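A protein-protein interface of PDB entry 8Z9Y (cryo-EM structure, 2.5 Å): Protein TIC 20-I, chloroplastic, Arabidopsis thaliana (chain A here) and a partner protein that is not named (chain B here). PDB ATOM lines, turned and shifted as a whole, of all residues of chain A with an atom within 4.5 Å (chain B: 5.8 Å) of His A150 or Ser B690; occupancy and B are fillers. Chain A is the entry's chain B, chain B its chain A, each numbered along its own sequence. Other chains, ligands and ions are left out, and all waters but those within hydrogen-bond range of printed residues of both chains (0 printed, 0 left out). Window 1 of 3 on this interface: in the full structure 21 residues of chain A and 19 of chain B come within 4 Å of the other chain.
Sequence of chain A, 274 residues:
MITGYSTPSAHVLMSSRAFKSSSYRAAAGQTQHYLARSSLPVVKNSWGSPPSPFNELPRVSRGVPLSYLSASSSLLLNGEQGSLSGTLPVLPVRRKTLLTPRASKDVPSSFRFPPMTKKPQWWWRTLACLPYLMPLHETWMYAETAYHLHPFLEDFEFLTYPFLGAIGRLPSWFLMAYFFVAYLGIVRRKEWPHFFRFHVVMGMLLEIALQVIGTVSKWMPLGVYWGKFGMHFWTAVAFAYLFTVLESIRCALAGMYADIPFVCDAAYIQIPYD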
ATOM      1  N   ALA A 146     -12.890  19.373  34.119  1.00  0.00           N
ATOM      2  CA  ALA A 146     -12.840  20.782  33.755  1.00  0.00           C
ATOM      3  C   ALA A 146     -11.766  21.084  32.722  1.00  0.00           C
ATOM      4  O   ALA A 146     -11.614  22.247  32.332  1.00  0.00           O
ATOM      5  CB  ALA A 146     -12.612  21.638  35.002  1.00  0.00           C
ATOM      6  N   TYR A 147     -11.018  20.071  32.280  1.00  0.00           N
ATOM      7  CA  TYR A 147      -9.976  20.289  31.282  1.00  0.00           C
ATOM      8  C   TYR A 147     -10.557  20.760  29.956  1.00  0.00           C
ATOM      9  O   TYR A 147      -9.871  21.439  29.185  1.00  0.00           O
ATOM     10  CB  TYR A 147      -9.168  19.006  31.088  1.00  0.00           C
ATOM     11  CG  TYR A 147      -8.240  18.684  32.239  1.00  0.00           C
ATOM     12  CD1 TYR A 147      -8.214  19.473  33.381  1.00  0.00           C
ATOM     13  CD2 TYR A 147      -7.390  17.588  32.183  1.00  0.00           C
ATOM     14  CE1 TYR A 147      -7.368  19.182  34.432  1.00  0.00           C
ATOM     15  CE2 TYR A 147      -6.542  17.289  33.230  1.00  0.00           C
ATOM     16  CZ  TYR A 147      -6.535  18.088  34.352  1.00  0.00           C
ATOM     17  OH  TYR A 147      -5.692  17.795  35.398  1.00  0.00           O
ATOM     18  N   HIS A 148     -11.812  20.410  29.672  1.00  0.00           N
ATOM     19  CA  HIS A 148     -12.484  20.902  28.478  1.00  0.00           C
ATOM     20  C   HIS A 148     -12.827  22.382  28.570  1.00  0.00           C
ATOM     21  O   HIS A 148     -13.225  22.973  27.561  1.00  0.00           O
ATOM     22  CB  HIS A 148     -13.765  20.104  28.229  1.00  0.00           C
ATOM     23  CG  HIS A 148     -13.561  18.622  28.208  1.00  0.00           C
ATOM     24  ND1 HIS A 148     -14.305  17.759  28.983  1.00  0.00           N
ATOM     25  CD2 HIS A 148     -12.698  17.849  27.506  1.00  0.00           C
ATOM     26  CE1 HIS A 148     -13.909  16.518  28.759  1.00  0.00           C
ATOM     27  NE2 HIS A 148     -12.935  16.546  27.868  1.00  0.00           N
ATOM     28  N   LEU A 149     -12.684  22.988  29.746  1.00  0.00           N
ATOM     29  CA  LEU A 149     -13.141  24.348  30.002  1.00  0.00           C
ATOM     30  C   LEU A 149     -12.017  25.366  30.108  1.00  0.00           C
ATOM     31  O   LEU A 149     -12.155  26.479  29.599  1.00  0.00           O
ATOM     32  CB  LEU A 149     -13.973  24.378  31.288  1.00  0.00           C
ATOM     33  CG  LEU A 149     -14.829  25.614  31.557  1.00  0.00           C
ATOM     34  CD1 LEU A 149     -16.192  25.202  32.085  1.00  0.00           C
ATOM     35  CD2 LEU A 149     -14.135  26.541  32.542  1.00  0.00           C
ATOM     36  N   HIS A 150     -10.905  25.022  30.756  1.00  0.00           N
ATOM     37  CA  HIS A 150      -9.826  25.974  31.005  1.00  0.00           C
ATOM     38  C   HIS A 150      -8.499  25.365  30.575  1.00  0.00           C
ATOM     39  O   HIS A 150      -8.141  24.267  31.049  1.00  0.00           O
ATOM     40  CB  HIS A 150      -9.790  26.377  32.480  1.00  0.00           C
ATOM     41  CG  HIS A 150      -9.239  27.748  32.717  1.00  0.00           C
ATOM     42  ND1 HIS A 150      -7.906  28.054  32.549  1.00  0.00           N
ATOM     43  CD2 HIS A 150      -9.842  28.897  33.103  1.00  0.00           C
ATOM     44  CE1 HIS A 150      -7.710  29.330  32.827  1.00  0.00           C
ATOM     45  NE2 HIS A 150      -8.869  29.865  33.165  1.00  0.00           N
ATOM     46  N   PRO A 151      -7.744  26.020  29.689  1.00  0.00           N
ATOM     47  CA  PRO A 151      -6.456  25.451  29.264  1.00  0.00           C
ATOM     48  C   PRO A 151      -5.400  25.431  30.354  1.00  0.00           C
ATOM     49  O   PRO A 151      -4.515  24.566  30.319  1.00  0.00           O
ATOM     50  CB  PRO A 151      -6.041  26.363  28.102  1.00  0.00           C
ATOM     51  CG  PRO A 151      -6.737  27.652  28.372  1.00  0.00           C
ATOM     52  CD  PRO A 151      -8.053  27.277  28.989  1.00  0.00           C
ATOM     53  N   PHE A 152      -5.451  26.361  31.312  1.00  0.00           N
ATOM     54  CA  PHE A 152      -4.385  26.461  32.304  1.00  0.00           C
ATOM     55  C   PHE A 152      -4.300  25.214  33.176  1.00  0.00           C
ATOM     56  O   PHE A 152      -3.239  24.923  33.742  1.00  0.00           O
ATOM     57  CB  PHE A 152      -4.590  27.698  33.176  1.00  0.00           C
ATOM     58  CG  PHE A 152      -3.669  27.764  34.359  1.00  0.00           C
ATOM     59  CD1 PHE A 152      -2.319  28.020  34.186  1.00  0.00           C
ATOM     60  CD2 PHE A 152      -4.147  27.555  35.641  1.00  0.00           C
ATOM     61  CE1 PHE A 152      -1.467  28.078  35.271  1.00  0.00           C
ATOM     62  CE2 PHE A 152      -3.300  27.613  36.730  1.00  0.00           C
ATOM     63  CZ  PHE A 152      -1.957  27.873  36.544  1.00  0.00           C
ATOM     64  N   LEU A 153      -5.407  24.479  33.310  1.00  0.00           N
ATOM     65  CA  LEU A 153      -5.380  23.248  34.088  1.00  0.00           C
ATOM     66  C   LEU A 153      -4.474  22.206  33.447  1.00  0.00           C
ATOM     67  O   LEU A 153      -3.957  21.323  34.139  1.00  0.00           O
ATOM     68  CB  LEU A 153      -6.799  22.702  34.251  1.00  0.00           C
ATOM     69  CG  LEU A 153      -7.747  23.557  35.093  1.00  0.00           C
ATOM     70  CD1 LEU A 153      -8.996  22.773  35.460  1.00  0.00           C
ATOM     71  CD2 LEU A 153      -7.047  24.071  36.341  1.00  0.00           C
ATOM     72  N   GLU A 154      -4.273  22.289  32.129  1.00  0.00           N
ATOM     73  CA  GLU A 154      -3.325  21.398  31.470  1.00  0.00           C
ATOM     74  C   GLU A 154      -1.899  21.713  31.902  1.00  0.00           C
ATOM     75  O   GLU A 154      -1.140  20.815  32.286  1.00  0.00           O
ATOM     76  CB  GLU A 154      -3.454  21.515  29.951  1.00  0.00           C
ATOM     77  CG  GLU A 154      -4.868  21.372  29.417  1.00  0.00           C
ATOM     78  CD  GLU A 154      -5.706  20.404  30.221  1.00  0.00           C
ATOM     79  OE1 GLU A 154      -5.353  19.206  30.282  1.00  0.00           O
ATOM     80  OE2 GLU A 154      -6.712  20.851  30.803  1.00  0.00           O
ATOM     81  N   PHE A 239     -10.237  26.280  41.101  1.00  0.00           N
ATOM     82  CA  PHE A 239      -9.675  27.626  41.153  1.00  0.00           C
ATOM     83  C   PHE A 239      -9.785  28.219  42.552  1.00  0.00           C
ATOM     84  O   PHE A 239      -8.822  28.807  43.064  1.00  0.00           O
ATOM     85  CB  PHE A 239     -10.363  28.526  40.128  1.00  0.00           C
ATOM     86  CG  PHE A 239      -9.681  28.548  38.792  1.00  0.00           C
ATOM     87  CD1 PHE A 239      -8.373  28.988  38.676  1.00  0.00           C
ATOM     88  CD2 PHE A 239     -10.342  28.124  37.653  1.00  0.00           C
ATOM     89  CE1 PHE A 239      -7.739  29.008  37.449  1.00  0.00           C
ATOM     90  CE2 PHE A 239      -9.712  28.141  36.423  1.00  0.00           C
ATOM     91  CZ  PHE A 239      -8.410  28.584  36.321  1.00  0.00           C
ATOM     92  N   VAL B 237      -8.088  35.754  36.504  1.00  0.00           N
ATOM     93  CA  VAL B 237      -8.322  34.404  35.995  1.00  0.00           C
ATOM     94  C   VAL B 237      -8.448  34.418  34.476  1.00  0.00           C
ATOM     95  O   VAL B 237      -7.869  33.573  33.779  1.00  0.00           O
ATOM     96  CB  VAL B 237      -9.566  33.791  36.663  1.00  0.00           C
ATOM     97  CG1 VAL B 237     -10.026  32.557  35.903  1.00  0.00           C
ATOM     98  CG2 VAL B 237      -9.272  33.450  38.112  1.00  0.00           C
ATOM     99  N   TYR B 238      -9.201  35.383  33.938  1.00  0.00           N
ATOM    100  CA  TYR B 238      -9.387  35.462  32.493  1.00  0.00           C
ATOM    101  C   TYR B 238      -8.059  35.664  31.776  1.00  0.00           C
ATOM    102  O   TYR B 238      -7.794  35.019  30.753  1.00  0.00           O
ATOM    103  CB  TYR B 238     -10.353  36.596  32.151  1.00  0.00           C
ATOM    104  CG  TYR B 238     -11.705  36.129  31.664  1.00  0.00           C
ATOM    105  CD1 TYR B 238     -11.862  35.605  30.389  1.00  0.00           C
ATOM    106  CD2 TYR B 238     -12.827  36.219  32.479  1.00  0.00           C
ATOM    107  CE1 TYR B 238     -13.097  35.179  29.939  1.00  0.00           C
ATOM    108  CE2 TYR B 238     -14.066  35.795  32.036  1.00  0.00           C
ATOM    109  CZ  TYR B 238     -14.195  35.276  30.766  1.00  0.00           C
ATOM    110  OH  TYR B 238     -15.425  34.854  30.321  1.00  0.00           O
ATOM    111  N   LEU B 240      -5.073  34.869  33.005  1.00  0.00           N
ATOM    112  CA  LEU B 240      -4.317  33.640  33.212  1.00  0.00           C
ATOM    113  C   LEU B 240      -4.729  32.559  32.224  1.00  0.00           C
ATOM    114  O   LEU B 240      -3.918  31.696  31.872  1.00  0.00           O
ATOM    115  CB  LEU B 240      -4.493  33.173  34.659  1.00  0.00           C
ATOM    116  CG  LEU B 240      -4.043  31.780  35.094  1.00  0.00           C
ATOM    117  CD1 LEU B 240      -3.534  31.827  36.519  1.00  0.00           C
ATOM    118  CD2 LEU B 240      -5.205  30.810  34.997  1.00  0.00           C
ATOM    119  N   GLY B 241      -5.973  32.596  31.760  1.00  0.00           N
ATOM    120  CA  GLY B 241      -6.383  31.698  30.703  1.00  0.00           C
ATOM    121  C   GLY B 241      -5.954  32.103  29.312  1.00  0.00           C
ATOM    122  O   GLY B 241      -6.260  31.395  28.349  1.00  0.00           O
ATOM    123  N   PRO B 364      -5.551  21.702  18.813  1.00  0.00           N
ATOM    124  CA  PRO B 364      -5.892  20.293  19.078  1.00  0.00           C
ATOM    125  C   PRO B 364      -6.046  19.480  17.796  1.00  0.00           C
ATOM    126  O   PRO B 364      -7.110  18.933  17.495  1.00  0.00           O
ATOM    127  CB  PRO B 364      -7.205  20.419  19.861  1.00  0.00           C
ATOM    128  CG  PRO B 364      -7.827  21.666  19.338  1.00  0.00           C
ATOM    129  CD  PRO B 364      -6.693  22.606  19.034  1.00  0.00           C
ATOM    130  N   MET B 688      -4.646  23.139  23.966  1.00  0.00           N
ATOM    131  CA  MET B 688      -5.497  23.514  25.088  1.00  0.00           C
ATOM    132  C   MET B 688      -6.679  22.574  25.295  1.00  0.00           C
ATOM    133  O   MET B 688      -7.301  22.624  26.362  1.00  0.00           O
ATOM    134  CB  MET B 688      -6.000  24.947  24.900  1.00  0.00           C
ATOM    135  CG  MET B 688      -6.411  25.289  23.482  1.00  0.00           C
ATOM    136  SD  MET B 688      -6.282  27.059  23.161  1.00  0.00           S
ATOM    137  CE  MET B 688      -4.515  27.235  22.931  1.00  0.00           C
ATOM    138  N   ARG B 689      -7.024  21.757  24.294  1.00  0.00           N
ATOM    139  CA  ARG B 689      -8.056  20.727  24.412  1.00  0.00           C
ATOM    140  C   ARG B 689      -9.451  21.331  24.556  1.00  0.00           C
ATOM    141  O   ARG B 689     -10.452  20.606  24.554  1.00  0.00           O
ATOM    142  CB  ARG B 689      -7.744  19.797  25.594  1.00  0.00           C
ATOM    143  CG  ARG B 689      -8.604  18.547  25.693  1.00  0.00           C
ATOM    144  CD  ARG B 689      -8.244  17.737  26.924  1.00  0.00           C
ATOM    145  NE  ARG B 689      -9.302  16.807  27.298  1.00  0.00           N
ATOM    146  CZ  ARG B 689      -9.198  15.912  28.269  1.00  0.00           C
ATOM    147  NH1 ARG B 689      -8.095  15.801  28.992  1.00  0.00           N
ATOM    148  NH2 ARG B 689     -10.226  15.106  28.523  1.00  0.00           N
ATOM    149  N   SER B 690      -9.539  22.654  24.649  1.00  0.00           N
ATOM    150  CA  SER B 690     -10.806  23.329  24.891  1.00  0.00           C
ATOM    151  C   SER B 690     -11.512  23.760  23.613  1.00  0.00           C
ATOM    152  O   SER B 690     -12.623  24.296  23.692  1.00  0.00           O
ATOM    153  CB  SER B 690     -10.590  24.547  25.796  1.00  0.00           C
ATOM    154  OG  SER B 690     -10.002  24.169  27.028  1.00  0.00           O
ATOM    155  N   GLN B 691     -10.912  23.546  22.446  1.00  0.00           N
ATOM    156  CA  GLN B 691     -11.513  23.954  21.181  1.00  0.00           C
ATOM    157  C   GLN B 691     -11.423  22.830  20.156  1.00  0.00           C
ATOM    158  O   GLN B 691     -11.037  23.030  19.004  1.00  0.00           O
ATOM    159  CB  GLN B 691     -10.871  25.235  20.658  1.00  0.00           C
ATOM    160  CG  GLN B 691      -9.356  25.244  20.686  1.00  0.00           C
ATOM    161  CD  GLN B 691      -8.785  26.575  20.242  1.00  0.00           C
ATOM    162  OE1 GLN B 691      -9.074  27.054  19.146  1.00  0.00           O
ATOM    163  NE2 GLN B 691      -7.961  27.176  21.091  1.00  0.00           N
ATOM    164  N   ARG B 692     -11.775  21.619  20.578  1.00  0.00           N
ATOM    165  CA  ARG B 692     -12.022  20.548  19.624  1.00  0.00           C
ATOM    166  C   ARG B 692     -13.361  20.780  18.938  1.00  0.00           C
ATOM    167  O   ARG B 692     -14.310  21.279  19.548  1.00  0.00           O
ATOM    168  CB  ARG B 692     -12.015  19.188  20.321  1.00  0.00           C
ATOM    169  CG  ARG B 692     -10.715  18.843  21.023  1.00  0.00           C
ATOM    170  CD  ARG B 692     -10.965  17.893  22.183  1.00  0.00           C
ATOM    171  NE  ARG B 692      -9.978  16.822  22.238  1.00  0.00           N
ATOM    172  CZ  ARG B 692     -10.070  15.759  23.026  1.00  0.00           C
ATOM    173  NH1 ARG B 692     -11.094  15.594  23.846  1.00  0.00           N
ATOM    174  NH2 ARG B 692      -9.109  14.840  22.991  1.00  0.00           N
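NE2 of His A148 sits at hydrogen-bond distance from NH2 of Arg B689 (3.1 Å). The side-chain hydroxyl of Ser B690 is in hydrogen-bond range of the backbone carbonyl oxygen of His A148 (3.5 Å). The side-chain hydroxyl (OG) of Ser B690 sits at hydrogen-bond distance from the backbone carbonyl oxygen (O) of Tyr A147 (3.5 Å).
SD of Met B688 is in hydrogen-bond range of NE2 of Gln B691 (2.7 Å). The side-chain hydroxyl (OG) of Ser B690 is in hydrogen-bond range of the backbone carbonyl oxygen (O) of Met B688 (3.2 Å). The backbone NH (N) of Phe A152 lies within hydrogen-bond range of a ring nitrogen (ND1) of His A150 (3.2 Å).
Among the printed residues, merely in contact across the chains: His A150 with Gly B241, Phe A152 with Leu B240, Pro A151 with Met B688, His A150 with Leu B240, Tyr A147 with Arg B689, Pro A151 with Gly B241, Leu A149 with Ser B690, His A150 with Val B237, His A150 with Ser B690, Pro A151 with Ser B690, Phe A239 with Leu B240 and Tyr A147 with Met B688.
Of chain A, only Tyr A147, His A148, Leu A149, His A150 and Pro A151 come within 4 Å of Ser B690. Of the printed residues of chain B, Phe A152 touches Leu B240 (3.5 Å). Printed residues of chain B within 4 Å of Leu A149: Ser B690 (3.9 Å). Of the printed residues of chain A, Met B688 touches Tyr A147 (3.997 Å) and Pro A151 (3.5 Å).
Of the 10 printed residues of chain A, 7 touch a printed residue of chain B. Along chain A the printed residues that touch a printed residue of chain B span positions 147 to 239. Of the 10 printed residues of chain B, 6 touch a printed residue of chain A. Among the printed residues, no Asp or Glu carboxylate lies within 4 Å of a Lys or Arg side-chain nitrogen of the other chain.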
